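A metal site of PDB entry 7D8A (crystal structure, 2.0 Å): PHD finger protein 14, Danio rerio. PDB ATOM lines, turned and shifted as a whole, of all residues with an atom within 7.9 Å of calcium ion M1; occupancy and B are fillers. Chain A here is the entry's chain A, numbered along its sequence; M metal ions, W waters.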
ATOM      1  N   LEU A  76     -13.946 -16.570  -2.441  1.00  0.00           N
ATOM      2  CA  LEU A  76     -15.346 -16.986  -2.469  1.00  0.00           C
ATOM      3  C   LEU A  76     -16.296 -15.964  -3.093  1.00  0.00           C
ATOM      4  O   LEU A  76     -17.494 -16.248  -3.174  1.00  0.00           O
ATOM      5  CB  LEU A  76     -15.825 -17.306  -1.035  1.00  0.00           C
ATOM      6  CG  LEU A  76     -15.059 -18.413  -0.287  1.00  0.00           C
ATOM      7  CD1 LEU A  76     -15.592 -18.604   1.137  1.00  0.00           C
ATOM      8  CD2 LEU A  76     -15.124 -19.723  -1.043  1.00  0.00           C
ATOM      9  N   VAL A  95     -14.395 -12.554   6.076  1.00  0.00           N
ATOM     10  CA  VAL A  95     -15.020 -13.168   7.242  1.00  0.00           C
ATOM     11  C   VAL A  95     -16.469 -13.552   6.924  1.00  0.00           C
ATOM     12  O   VAL A  95     -16.905 -14.667   7.201  1.00  0.00           O
ATOM     13  CB  VAL A  95     -14.933 -12.228   8.450  1.00  0.00           C
ATOM     14  CG1 VAL A  95     -15.785 -12.757   9.603  1.00  0.00           C
ATOM     15  CG2 VAL A  95     -13.461 -12.089   8.889  1.00  0.00           C
ATOM     16  N   VAL A  96     -17.230 -12.623   6.326  1.00  0.00           N
ATOM     17  CA  VAL A  96     -18.649 -12.889   6.142  1.00  0.00           C
ATOM     18  C   VAL A  96     -18.870 -14.033   5.150  1.00  0.00           C
ATOM     19  O   VAL A  96     -19.755 -14.878   5.334  1.00  0.00           O
ATOM     20  CB  VAL A  96     -19.403 -11.596   5.749  1.00  0.00           C
ATOM     21  CG1 VAL A  96     -19.010 -11.078   4.371  1.00  0.00           C
ATOM     22  CG2 VAL A  96     -20.911 -11.793   5.827  1.00  0.00           C
ATOM     23  N   CYS A  97     -18.019 -14.126   4.113  1.00  0.00           N
ATOM     24  CA  CYS A  97     -18.130 -15.272   3.199  1.00  0.00           C
ATOM     25  C   CYS A  97     -17.870 -16.575   3.923  1.00  0.00           C
ATOM     26  O   CYS A  97     -18.598 -17.564   3.723  1.00  0.00           O
ATOM     27  CB  CYS A  97     -17.184 -15.115   2.018  1.00  0.00           C
ATOM     28  SG  CYS A  97     -17.728 -13.906   0.808  1.00  0.00           S
ATOM     29  N   ALA A  98     -16.849 -16.615   4.779  1.00  0.00           N
ATOM     30  CA  ALA A  98     -16.530 -17.859   5.490  1.00  0.00           C
ATOM     31  C   ALA A  98     -17.657 -18.256   6.436  1.00  0.00           C
ATOM     32  O   ALA A  98     -17.939 -19.446   6.593  1.00  0.00           O
ATOM     33  CB  ALA A  98     -15.232 -17.692   6.275  1.00  0.00           C
ATOM     34  N   LEU A  99     -18.317 -17.281   7.055  1.00  0.00           N
ATOM     35  CA  LEU A  99     -19.416 -17.594   7.965  1.00  0.00           C
ATOM     36  C   LEU A  99     -20.588 -18.244   7.224  1.00  0.00           C
ATOM     37  O   LEU A  99     -21.135 -19.256   7.672  1.00  0.00           O
ATOM     38  CB  LEU A  99     -19.896 -16.337   8.682  1.00  0.00           C
ATOM     39  CG  LEU A  99     -18.930 -15.721   9.693  1.00  0.00           C
ATOM     40  CD1 LEU A  99     -19.481 -14.410  10.223  1.00  0.00           C
ATOM     41  CD2 LEU A  99     -18.662 -16.684  10.845  1.00  0.00           C
ATOM     42  N   TYR A 100     -20.968 -17.662   6.083  1.00  0.00           N
ATOM     43  CA  TYR A 100     -22.214 -18.017   5.423  1.00  0.00           C
ATOM     44  C   TYR A 100     -22.069 -19.160   4.416  1.00  0.00           C
ATOM     45  O   TYR A 100     -23.056 -19.873   4.154  1.00  0.00           O
ATOM     46  CB  TYR A 100     -22.810 -16.767   4.742  1.00  0.00           C
ATOM     47  CG  TYR A 100     -23.551 -15.868   5.746  1.00  0.00           C
ATOM     48  CD1 TYR A 100     -24.922 -15.995   5.957  1.00  0.00           C
ATOM     49  CD2 TYR A 100     -22.865 -14.913   6.497  1.00  0.00           C
ATOM     50  CE1 TYR A 100     -25.594 -15.213   6.884  1.00  0.00           C
ATOM     51  CE2 TYR A 100     -23.531 -14.109   7.428  1.00  0.00           C
ATOM     52  CZ  TYR A 100     -24.897 -14.260   7.605  1.00  0.00           C
ATOM     53  OH  TYR A 100     -25.581 -13.490   8.518  1.00  0.00           O
ATOM     54  N   VAL A 101     -20.885 -19.396   3.870  1.00  0.00           N
ATOM     55  CA  VAL A 101     -20.748 -20.462   2.872  1.00  0.00           C
ATOM     56  C   VAL A 101     -20.665 -21.816   3.583  1.00  0.00           C
ATOM     57  O   VAL A 101     -19.841 -21.968   4.505  1.00  0.00           O
ATOM     58  CB  VAL A 101     -19.537 -20.220   1.979  1.00  0.00           C
ATOM     59  CG1 VAL A 101     -19.208 -21.489   1.176  1.00  0.00           C
ATOM     60  CG2 VAL A 101     -19.812 -19.035   1.021  1.00  0.00           C
ATOM     61  N   PRO A 102     -21.487 -22.789   3.207  1.00  0.00           N
ATOM     62  CA  PRO A 102     -21.425 -24.094   3.870  1.00  0.00           C
ATOM     63  C   PRO A 102     -20.089 -24.795   3.659  1.00  0.00           C
ATOM     64  O   PRO A 102     -19.422 -24.664   2.626  1.00  0.00           O
ATOM     65  CB  PRO A 102     -22.578 -24.893   3.233  1.00  0.00           C
ATOM     66  CG  PRO A 102     -23.070 -24.112   2.083  1.00  0.00           C
ATOM     67  CD  PRO A 102     -22.506 -22.708   2.153  1.00  0.00           C
ATOM     68  N   GLY A 103     -19.675 -25.544   4.669  1.00  0.00           N
ATOM     69  CA  GLY A 103     -18.472 -26.293   4.534  1.00  0.00           C
ATOM     70  C   GLY A 103     -17.219 -25.497   4.746  1.00  0.00           C
ATOM     71  O   GLY A 103     -16.127 -26.019   4.503  1.00  0.00           O
ATOM     72  N   VAL A 104     -17.340 -24.237   5.171  1.00  0.00           N
ATOM     73  CA  VAL A 104     -16.196 -23.395   5.496  1.00  0.00           C
ATOM     74  C   VAL A 104     -16.264 -23.103   6.987  1.00  0.00           C
ATOM     75  O   VAL A 104     -17.304 -22.681   7.490  1.00  0.00           O
ATOM     76  CB  VAL A 104     -16.169 -22.102   4.671  1.00  0.00           C
ATOM     77  CG1 VAL A 104     -14.949 -21.253   5.060  1.00  0.00           C
ATOM     78  CG2 VAL A 104     -16.162 -22.441   3.205  1.00  0.00           C
ATOM     79  N   ALA A 105     -15.186 -23.400   7.693  1.00  0.00           N
ATOM     80  CA  ALA A 105     -15.133 -23.270   9.129  1.00  0.00           C
ATOM     81  C   ALA A 105     -13.828 -22.577   9.519  1.00  0.00           C
ATOM     82  O   ALA A 105     -12.843 -22.617   8.776  1.00  0.00           O
ATOM     83  CB  ALA A 105     -15.226 -24.645   9.820  1.00  0.00           C
ATOM     84  N   PHE A 106     -13.838 -21.961  10.687  1.00  0.00           N
ATOM     85  CA  PHE A 106     -12.631 -21.350  11.245  1.00  0.00           C
ATOM     86  C   PHE A 106     -11.865 -22.370  12.087  1.00  0.00           C
ATOM     87  O   PHE A 106     -12.448 -23.116  12.873  1.00  0.00           O
ATOM     88  CB  PHE A 106     -12.987 -20.137  12.086  1.00  0.00           C
ATOM     89  CG  PHE A 106     -13.568 -19.001  11.300  1.00  0.00           C
ATOM     90  CD1 PHE A 106     -12.755 -17.976  10.844  1.00  0.00           C
ATOM     91  CD2 PHE A 106     -14.918 -18.958  11.007  1.00  0.00           C
ATOM     92  CE1 PHE A 106     -13.286 -16.931  10.103  1.00  0.00           C
ATOM     93  CE2 PHE A 106     -15.435 -17.914  10.268  1.00  0.00           C
ATOM     94  CZ  PHE A 106     -14.609 -16.890   9.824  1.00  0.00           C
ATOM     95  N   ASN A 121     -14.995 -27.099  -1.278  1.00  0.00           N
ATOM     96  CA  ASN A 121     -15.262 -25.668  -1.484  1.00  0.00           C
ATOM     97  C   ASN A 121     -14.886 -25.252  -2.900  1.00  0.00           C
ATOM     98  O   ASN A 121     -15.643 -24.561  -3.583  1.00  0.00           O
ATOM     99  CB  ASN A 121     -14.487 -24.804  -0.478  1.00  0.00           C
ATOM    100  CG  ASN A 121     -14.808 -25.137   0.958  1.00  0.00           C
ATOM    101  OD1 ASN A 121     -13.936 -25.114   1.810  1.00  0.00           O
ATOM    102  ND2 ASN A 121     -16.066 -25.462   1.220  1.00  0.00           N
ATOM    103  N   ASP A 178     -26.547 -23.836  12.845  1.00  0.00           N
ATOM    104  CA  ASP A 178     -25.996 -22.869  11.902  1.00  0.00           C
ATOM    105  C   ASP A 178     -26.839 -21.603  12.002  1.00  0.00           C
ATOM    106  O   ASP A 178     -27.890 -21.519  11.342  1.00  0.00           O
ATOM    107  CB  ASP A 178     -26.011 -23.414  10.474  1.00  0.00           C
ATOM    108  CG  ASP A 178     -25.532 -22.393   9.445  1.00  0.00           C
ATOM    109  OD1 ASP A 178     -24.887 -21.371   9.811  1.00  0.00           O
ATOM    110  OD2 ASP A 178     -25.779 -22.629   8.240  1.00  0.00           O
ATOM    111  N   PHE A 180     -26.376 -18.671  10.781  1.00  0.00           N
ATOM    112  CA  PHE A 180     -26.215 -17.743   9.670  1.00  0.00           C
ATOM    113  C   PHE A 180     -27.068 -18.206   8.493  1.00  0.00           C
ATOM    114  O   PHE A 180     -26.918 -19.338   8.019  1.00  0.00           O
ATOM    115  CB  PHE A 180     -24.730 -17.631   9.270  1.00  0.00           C
ATOM    116  CG  PHE A 180     -23.823 -17.228  10.426  1.00  0.00           C
ATOM    117  CD1 PHE A 180     -23.790 -15.927  10.880  1.00  0.00           C
ATOM    118  CD2 PHE A 180     -23.000 -18.180  11.041  1.00  0.00           C
ATOM    119  CE1 PHE A 180     -22.971 -15.557  11.947  1.00  0.00           C
ATOM    120  CE2 PHE A 180     -22.166 -17.824  12.108  1.00  0.00           C
ATOM    121  CZ  PHE A 180     -22.148 -16.522  12.560  1.00  0.00           C
HETATM  122 CA    CA M   1     -19.325 -21.372   7.058  1.00  0.00          CA
HETATM  123 CA    CA M   2     -25.880 -20.766   6.588  1.00  0.00          CA
HETATM  124  O   HOH W   1     -20.562 -20.566   9.863  1.00  0.00           O
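Four residues have an atom within 4 Å of calcium ion M1: Ala 98, Leu 99, Val 101 and Val 104.
Calcium ion M1 is bound by the backbone carbonyl oxygen (O) of Ala 98, the backbone carbonyl oxygen (O) of Val 104, the backbone carbonyl oxygen (O) of Val 101 and the backbone carbonyl oxygen (O) of Leu 99.
Calcium ion M1 has four donor atoms within binding distance.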
